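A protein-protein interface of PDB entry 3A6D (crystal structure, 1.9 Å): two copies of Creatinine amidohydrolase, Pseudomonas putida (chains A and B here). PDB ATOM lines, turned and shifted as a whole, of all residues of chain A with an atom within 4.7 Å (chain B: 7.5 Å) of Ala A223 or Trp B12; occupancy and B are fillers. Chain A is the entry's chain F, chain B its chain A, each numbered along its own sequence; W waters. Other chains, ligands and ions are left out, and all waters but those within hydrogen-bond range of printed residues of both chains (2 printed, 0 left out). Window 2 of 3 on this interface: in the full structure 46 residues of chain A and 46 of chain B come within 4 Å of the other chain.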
ATOM      1  N   GLN A  35      12.369  13.431  24.902  1.00  0.00           N
ATOM      2  CA  GLN A  35      13.279  12.328  24.633  1.00  0.00           C
ATOM      3  C   GLN A  35      12.786  11.087  25.370  1.00  0.00           C
ATOM      4  O   GLN A  35      12.300  11.179  26.500  1.00  0.00           O
ATOM      5  CB  GLN A  35      14.696  12.681  25.102  1.00  0.00           C
ATOM      6  CG  GLN A  35      14.868  12.836  26.622  1.00  0.00           C
ATOM      7  CD  GLN A  35      14.968  11.503  27.359  1.00  0.00           C
ATOM      8  OE1 GLN A  35      15.285  10.472  26.762  1.00  0.00           O
ATOM      9  NE2 GLN A  35      14.714  11.527  28.667  1.00  0.00           N
ATOM     10  N   HIS A  36      12.899   9.935  24.716  1.00  0.00           N
ATOM     11  CA  HIS A  36      12.484   8.671  25.306  1.00  0.00           C
ATOM     12  C   HIS A  36      13.501   7.568  25.028  1.00  0.00           C
ATOM     13  O   HIS A  36      13.142   6.491  24.557  1.00  0.00           O
ATOM     14  CB  HIS A  36      11.116   8.241  24.773  1.00  0.00           C
ATOM     15  CG  HIS A  36       9.962   8.881  25.480  1.00  0.00           C
ATOM     16  ND1 HIS A  36       9.627  10.208  25.313  1.00  0.00           N
ATOM     17  CD2 HIS A  36       9.077   8.377  26.372  1.00  0.00           C
ATOM     18  CE1 HIS A  36       8.583  10.493  26.072  1.00  0.00           C
ATOM     19  NE2 HIS A  36       8.232   9.400  26.725  1.00  0.00           N
ATOM     20  N   GLY A  37      14.769   7.846  25.314  1.00  0.00           N
ATOM     21  CA  GLY A  37      15.809   6.855  25.104  1.00  0.00           C
ATOM     22  C   GLY A  37      16.271   6.701  23.667  1.00  0.00           C
ATOM     23  O   GLY A  37      15.832   7.426  22.775  1.00  0.00           O
ATOM     24  N   HIS A  38      17.161   5.738  23.448  1.00  0.00           N
ATOM     25  CA  HIS A  38      17.710   5.474  22.120  1.00  0.00           C
ATOM     26  C   HIS A  38      16.807   4.582  21.278  1.00  0.00           C
ATOM     27  O   HIS A  38      16.992   4.480  20.067  1.00  0.00           O
ATOM     28  CB  HIS A  38      19.071   4.770  22.235  1.00  0.00           C
ATOM     29  CG  HIS A  38      20.119   5.564  22.949  1.00  0.00           C
ATOM     30  ND1 HIS A  38      21.405   5.097  23.127  1.00  0.00           N
ATOM     31  CD2 HIS A  38      20.082   6.791  23.518  1.00  0.00           C
ATOM     32  CE1 HIS A  38      22.116   6.005  23.772  1.00  0.00           C
ATOM     33  NE2 HIS A  38      21.336   7.043  24.021  1.00  0.00           N
ATOM     34  N   MET A  42      10.012  10.517  20.117  1.00  0.00           N
ATOM     35  CA  MET A  42       9.708  11.546  21.108  1.00  0.00           C
ATOM     36  C   MET A  42       8.264  12.006  21.323  1.00  0.00           C
ATOM     37  O   MET A  42       8.011  12.805  22.227  1.00  0.00           O
ATOM     38  CB  MET A  42      10.595  12.769  20.838  1.00  0.00           C
ATOM     39  CG  MET A  42      12.092  12.450  20.863  1.00  0.00           C
ATOM     40  SD  MET A  42      13.144  13.905  20.765  1.00  0.00           S
ATOM     41  CE  MET A  42      13.148  14.196  18.995  1.00  0.00           C
ATOM     42  N   PHE A  84      18.066  17.603  27.724  1.00  0.00           N
ATOM     43  CA  PHE A  84      18.229  16.781  26.525  1.00  0.00           C
ATOM     44  C   PHE A  84      17.787  17.483  25.248  1.00  0.00           C
ATOM     45  O   PHE A  84      16.932  18.371  25.273  1.00  0.00           O
ATOM     46  CB  PHE A  84      17.419  15.481  26.623  1.00  0.00           C
ATOM     47  CG  PHE A  84      18.036  14.431  27.498  1.00  0.00           C
ATOM     48  CD1 PHE A  84      17.910  14.492  28.882  1.00  0.00           C
ATOM     49  CD2 PHE A  84      18.740  13.369  26.935  1.00  0.00           C
ATOM     50  CE1 PHE A  84      18.476  13.507  29.697  1.00  0.00           C
ATOM     51  CE2 PHE A  84      19.310  12.379  27.742  1.00  0.00           C
ATOM     52  CZ  PHE A  84      19.177  12.451  29.126  1.00  0.00           C
ATOM     53  N   PRO A  85      18.372  17.091  24.105  1.00  0.00           N
ATOM     54  CA  PRO A  85      18.007  17.684  22.819  1.00  0.00           C
ATOM     55  C   PRO A  85      16.646  17.080  22.486  1.00  0.00           C
ATOM     56  O   PRO A  85      16.278  16.050  23.053  1.00  0.00           O
ATOM     57  CB  PRO A  85      19.080  17.152  21.861  1.00  0.00           C
ATOM     58  CG  PRO A  85      20.229  16.770  22.768  1.00  0.00           C
ATOM     59  CD  PRO A  85      19.526  16.186  23.960  1.00  0.00           C
ATOM     60  N   THR A 221      21.387  11.473  35.559  1.00  0.00           N
ATOM     61  CA  THR A 221      20.366  10.807  34.756  1.00  0.00           C
ATOM     62  C   THR A 221      21.062   9.748  33.908  1.00  0.00           C
ATOM     63  O   THR A 221      22.141   9.995  33.373  1.00  0.00           O
ATOM     64  CB  THR A 221      19.667  11.789  33.778  1.00  0.00           C
ATOM     65  OG1 THR A 221      18.894  12.745  34.512  1.00  0.00           O
ATOM     66  CG2 THR A 221      18.759  11.027  32.813  1.00  0.00           C
ATOM     67  N   PRO A 222      20.470   8.549  33.788  1.00  0.00           N
ATOM     68  CA  PRO A 222      21.130   7.531  32.964  1.00  0.00           C
ATOM     69  C   PRO A 222      21.394   8.104  31.569  1.00  0.00           C
ATOM     70  O   PRO A 222      20.523   8.745  30.975  1.00  0.00           O
ATOM     71  CB  PRO A 222      20.117   6.395  32.954  1.00  0.00           C
ATOM     72  CG  PRO A 222      19.531   6.484  34.331  1.00  0.00           C
ATOM     73  CD  PRO A 222      19.311   7.981  34.498  1.00  0.00           C
ATOM     74  N   ALA A 223      22.597   7.871  31.056  1.00  0.00           N
ATOM     75  CA  ALA A 223      23.009   8.379  29.749  1.00  0.00           C
ATOM     76  C   ALA A 223      21.962   8.326  28.634  1.00  0.00           C
ATOM     77  O   ALA A 223      21.787   9.300  27.902  1.00  0.00           O
ATOM     78  CB  ALA A 223      24.281   7.660  29.297  1.00  0.00           C
ATOM     79  N   PRO A 224      21.263   7.192  28.481  1.00  0.00           N
ATOM     80  CA  PRO A 224      20.242   7.052  27.433  1.00  0.00           C
ATOM     81  C   PRO A 224      19.049   8.003  27.569  1.00  0.00           C
ATOM     82  O   PRO A 224      18.396   8.329  26.579  1.00  0.00           O
ATOM     83  CB  PRO A 224      19.809   5.590  27.563  1.00  0.00           C
ATOM     84  CG  PRO A 224      21.026   4.920  28.136  1.00  0.00           C
ATOM     85  CD  PRO A 224      21.468   5.908  29.177  1.00  0.00           C
ATOM     86  N   GLY A 225      18.766   8.435  28.794  1.00  0.00           N
ATOM     87  CA  GLY A 225      17.638   9.323  29.019  1.00  0.00           C
ATOM     88  C   GLY A 225      16.481   8.585  29.672  1.00  0.00           C
ATOM     89  O   GLY A 225      15.558   9.200  30.205  1.00  0.00           O
ATOM     90  N   VAL B   7       9.787  15.294  13.615  1.00  0.00           N
ATOM     91  CA  VAL B   7      10.604  15.258  14.822  1.00  0.00           C
ATOM     92  C   VAL B   7      10.024  14.293  15.856  1.00  0.00           C
ATOM     93  O   VAL B   7      10.758  13.557  16.516  1.00  0.00           O
ATOM     94  CB  VAL B   7      10.701  16.664  15.456  1.00  0.00           C
ATOM     95  CG1 VAL B   7      11.430  16.594  16.790  1.00  0.00           C
ATOM     96  CG2 VAL B   7      11.420  17.609  14.499  1.00  0.00           C
ATOM     97  N   LEU B  10      11.121  10.680  15.607  1.00  0.00           N
ATOM     98  CA  LEU B  10      12.557  10.413  15.695  1.00  0.00           C
ATOM     99  C   LEU B  10      12.949  10.209  17.155  1.00  0.00           C
ATOM    100  O   LEU B  10      12.216  10.616  18.054  1.00  0.00           O
ATOM    101  CB  LEU B  10      13.363  11.602  15.163  1.00  0.00           C
ATOM    102  CG  LEU B  10      13.194  12.064  13.716  1.00  0.00           C
ATOM    103  CD1 LEU B  10      14.121  13.249  13.464  1.00  0.00           C
ATOM    104  CD2 LEU B  10      13.518  10.925  12.769  1.00  0.00           C
ATOM    105  N   THR B  11      14.104   9.584  17.386  1.00  0.00           N
ATOM    106  CA  THR B  11      14.614   9.394  18.746  1.00  0.00           C
ATOM    107  C   THR B  11      15.397  10.677  19.012  1.00  0.00           C
ATOM    108  O   THR B  11      15.738  11.391  18.071  1.00  0.00           O
ATOM    109  CB  THR B  11      15.599   8.210  18.842  1.00  0.00           C
ATOM    110  OG1 THR B  11      16.790   8.519  18.107  1.00  0.00           O
ATOM    111  CG2 THR B  11      14.971   6.945  18.277  1.00  0.00           C
ATOM    112  N   TRP B  12      15.694  10.984  20.271  1.00  0.00           N
ATOM    113  CA  TRP B  12      16.431  12.210  20.537  1.00  0.00           C
ATOM    114  C   TRP B  12      17.836  12.155  19.945  1.00  0.00           C
ATOM    115  O   TRP B  12      18.413  13.189  19.607  1.00  0.00           O
ATOM    116  CB  TRP B  12      16.499  12.507  22.041  1.00  0.00           C
ATOM    117  CG  TRP B  12      17.384  11.606  22.855  1.00  0.00           C
ATOM    118  CD1 TRP B  12      17.022  10.448  23.486  1.00  0.00           C
ATOM    119  CD2 TRP B  12      18.752  11.844  23.209  1.00  0.00           C
ATOM    120  NE1 TRP B  12      18.076   9.960  24.222  1.00  0.00           N
ATOM    121  CE2 TRP B  12      19.151  10.795  24.070  1.00  0.00           C
ATOM    122  CE3 TRP B  12      19.680  12.845  22.886  1.00  0.00           C
ATOM    123  CZ2 TRP B  12      20.436  10.720  24.613  1.00  0.00           C
ATOM    124  CZ3 TRP B  12      20.960  12.769  23.426  1.00  0.00           C
ATOM    125  CH2 TRP B  12      21.326  11.712  24.282  1.00  0.00           C
ATOM    126  N   LYS B  13      18.383  10.949  19.812  1.00  0.00           N
ATOM    127  CA  LYS B  13      19.722  10.787  19.246  1.00  0.00           C
ATOM    128  C   LYS B  13      19.706  11.151  17.765  1.00  0.00           C
ATOM    129  O   LYS B  13      20.611  11.824  17.270  1.00  0.00           O
ATOM    130  CB  LYS B  13      20.200   9.342  19.411  1.00  0.00           C
ATOM    131  CG  LYS B  13      20.354   8.909  20.857  1.00  0.00           C
ATOM    132  CD  LYS B  13      21.503   9.633  21.544  1.00  0.00           C
ATOM    133  CE  LYS B  13      22.848   9.152  21.027  1.00  0.00           C
ATOM    134  NZ  LYS B  13      23.983   9.776  21.767  1.00  0.00           N
ATOM    135  N   GLU B  14      18.676  10.695  17.063  1.00  0.00           N
ATOM    136  CA  GLU B  14      18.534  10.974  15.638  1.00  0.00           C
ATOM    137  C   GLU B  14      18.339  12.475  15.413  1.00  0.00           C
ATOM    138  O   GLU B  14      18.927  13.057  14.505  1.00  0.00           O
ATOM    139  CB  GLU B  14      17.350  10.180  15.071  1.00  0.00           C
ATOM    140  CG  GLU B  14      17.593   8.665  15.056  1.00  0.00           C
ATOM    141  CD  GLU B  14      16.338   7.840  14.793  1.00  0.00           C
ATOM    142  OE1 GLU B  14      16.480   6.619  14.547  1.00  0.00           O
ATOM    143  OE2 GLU B  14      15.218   8.395  14.843  1.00  0.00           O
ATOM    144  N   TYR B  15      17.516  13.098  16.250  1.00  0.00           N
ATOM    145  CA  TYR B  15      17.265  14.533  16.145  1.00  0.00           C
ATOM    146  C   TYR B  15      18.564  15.293  16.425  1.00  0.00           C
ATOM    147  O   TYR B  15      18.931  16.219  15.700  1.00  0.00           O
ATOM    148  CB  TYR B  15      16.190  14.943  17.156  1.00  0.00           C
ATOM    149  CG  TYR B  15      15.963  16.433  17.244  1.00  0.00           C
ATOM    150  CD1 TYR B  15      15.170  17.097  16.305  1.00  0.00           C
ATOM    151  CD2 TYR B  15      16.557  17.184  18.255  1.00  0.00           C
ATOM    152  CE1 TYR B  15      14.973  18.477  16.374  1.00  0.00           C
ATOM    153  CE2 TYR B  15      16.370  18.563  18.333  1.00  0.00           C
ATOM    154  CZ  TYR B  15      15.577  19.198  17.391  1.00  0.00           C
ATOM    155  OH  TYR B  15      15.383  20.554  17.479  1.00  0.00           O
ATOM    156  N   GLU B  16      19.264  14.888  17.481  1.00  0.00           N
ATOM    157  CA  GLU B  16      20.521  15.527  17.847  1.00  0.00           C
ATOM    158  C   GLU B  16      21.509  15.513  16.682  1.00  0.00           C
ATOM    159  O   GLU B  16      22.153  16.521  16.382  1.00  0.00           O
ATOM    160  CB  GLU B  16      21.143  14.807  19.042  1.00  0.00           C
ATOM    161  CG  GLU B  16      22.390  15.476  19.584  1.00  0.00           C
ATOM    162  CD  GLU B  16      23.014  14.688  20.716  1.00  0.00           C
ATOM    163  OE1 GLU B  16      23.497  15.317  21.676  1.00  0.00           O
ATOM    164  OE2 GLU B  16      23.027  13.440  20.641  1.00  0.00           O
ATOM    165  N   ALA B  17      21.623  14.361  16.030  1.00  0.00           N
ATOM    166  CA  ALA B  17      22.541  14.204  14.906  1.00  0.00           C
ATOM    167  C   ALA B  17      22.182  15.139  13.755  1.00  0.00           C
ATOM    168  O   ALA B  17      23.062  15.742  13.139  1.00  0.00           O
ATOM    169  CB  ALA B  17      22.532  12.755  14.429  1.00  0.00           C
ATOM    170  N   ARG B  18      20.889  15.261  13.471  1.00  0.00           N
ATOM    171  CA  ARG B  18      20.430  16.129  12.398  1.00  0.00           C
ATOM    172  C   ARG B  18      20.760  17.583  12.686  1.00  0.00           C
ATOM    173  O   ARG B  18      21.213  18.305  11.800  1.00  0.00           O
ATOM    174  CB  ARG B  18      18.921  15.960  12.174  1.00  0.00           C
ATOM    175  CG  ARG B  18      18.553  14.652  11.494  1.00  0.00           C
ATOM    176  CD  ARG B  18      19.180  14.576  10.104  1.00  0.00           C
ATOM    177  NE  ARG B  18      18.513  15.462   9.153  1.00  0.00           N
ATOM    178  CZ  ARG B  18      17.371  15.167   8.539  1.00  0.00           C
ATOM    179  NH1 ARG B  18      16.771  14.006   8.770  1.00  0.00           N
ATOM    180  NH2 ARG B  18      16.822  16.033   7.699  1.00  0.00           N
HETATM  181  O   HOH W   1      18.417   6.329  18.611  1.00  0.00           O
HETATM  182  O   HOH W   2      13.984   9.344  22.109  1.00  0.00           O
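The indole nitrogen (NE1) of Trp B12 sits at hydrogen-bond distance from the backbone carbonyl oxygen (O) of Pro A224 (2.9 Å). The backbone carbonyl oxygen of Leu B10 is in hydrogen-bond range of the backbone NH of Met A42, 3.0 Å away.
The backbone NH of Lys B13 lies close to the side-chain hydroxyl of Thr B11, at 3.4 Å. The side-chain amide oxygen of Gln A35 is in hydrogen-bond range of the backbone NH of Gly A37. The side-chain amino group (NZ) of Lys B13 lies within salt-bridge range of the side-chain carboxylate (OE2) of Glu B16 (3.95 Å). N of Thr B11 sits at hydrogen-bond distance from OE2 of Glu B14 (3.0 Å). NE2 of Gln A35 sits at hydrogen-bond distance from O of Gly A225 (2.9 Å).
Among the printed residues, merely in contact across the chains: Gln A35 with Trp B12, Gly A37 with Trp B12, His A38 with Thr B11, His A38 with Trp B12, His A38 with Lys B13, Met A42 with Val B7, Met A42 with Thr B11, Met A42 with Trp B12, Met A42 with Tyr B15, Phe A84 with Trp B12, Pro A85 with Trp B12, Pro A85 with Glu B16 and Ala A223 with Trp B12.
Ala A223 touches just one residue of chain B: Trp B12. Of chain A, only Gln A35, Gly A37, His A38, Met A42, Phe A84, Pro A85, Ala A223 and Pro A224 come within 4 Å of Trp B12. Printed residues of chain B within 4 Å of His A38: Thr B11 (3.7 Å), Trp B12 (3.8 Å) and Lys B13 (3.4 Å). Of the printed residues of chain B, Pro A85 touches Trp B12 (3.5 Å) and Glu B16 (3.7 Å). Printed residues of chain A within 4 Å of Lys B13: His A38. Of the printed residues of chain A, Val B7 touches Met A42 (3.5 Å). Of the printed residues of chain A, Tyr B15 touches Met A42 (3.6 Å). Ala B17 touches none of the printed residues of chain A.
Of the 12 printed residues of chain A, 8 touch a printed residue of chain B. Hydrophobic or aromatic side chains of chain A within 4 Å of the printed part of chain B: His A38, Met A42, Phe A84 and Pro A85. Hydrophobic or aromatic side chains of chain B within 4 Å of the printed part of chain A: Val B7, Trp B12 and Tyr B15. Along chain B the printed residues that touch a printed residue of chain A span positions 7 to 16. Among the printed residues, no Asp or Glu carboxylate lies within 4 Å of a Lys or Arg side-chain nitrogen of the other chain.
No position is printed for both chains. Of the 15 pairs that touch across the chains among the printed residues, none has its exchanged pair printed and touching as well.
Water W2 lies within hydrogen-bond range of the backbone carbonyl oxygen (O) of Gly A37 (2.7 Å), the backbone NH (N) of His A36 (2.9 Å) and the backbone NH (N) of Trp B12 (3.0 Å). Water W1 bridges O of His A38 and OG1 of Thr B11.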
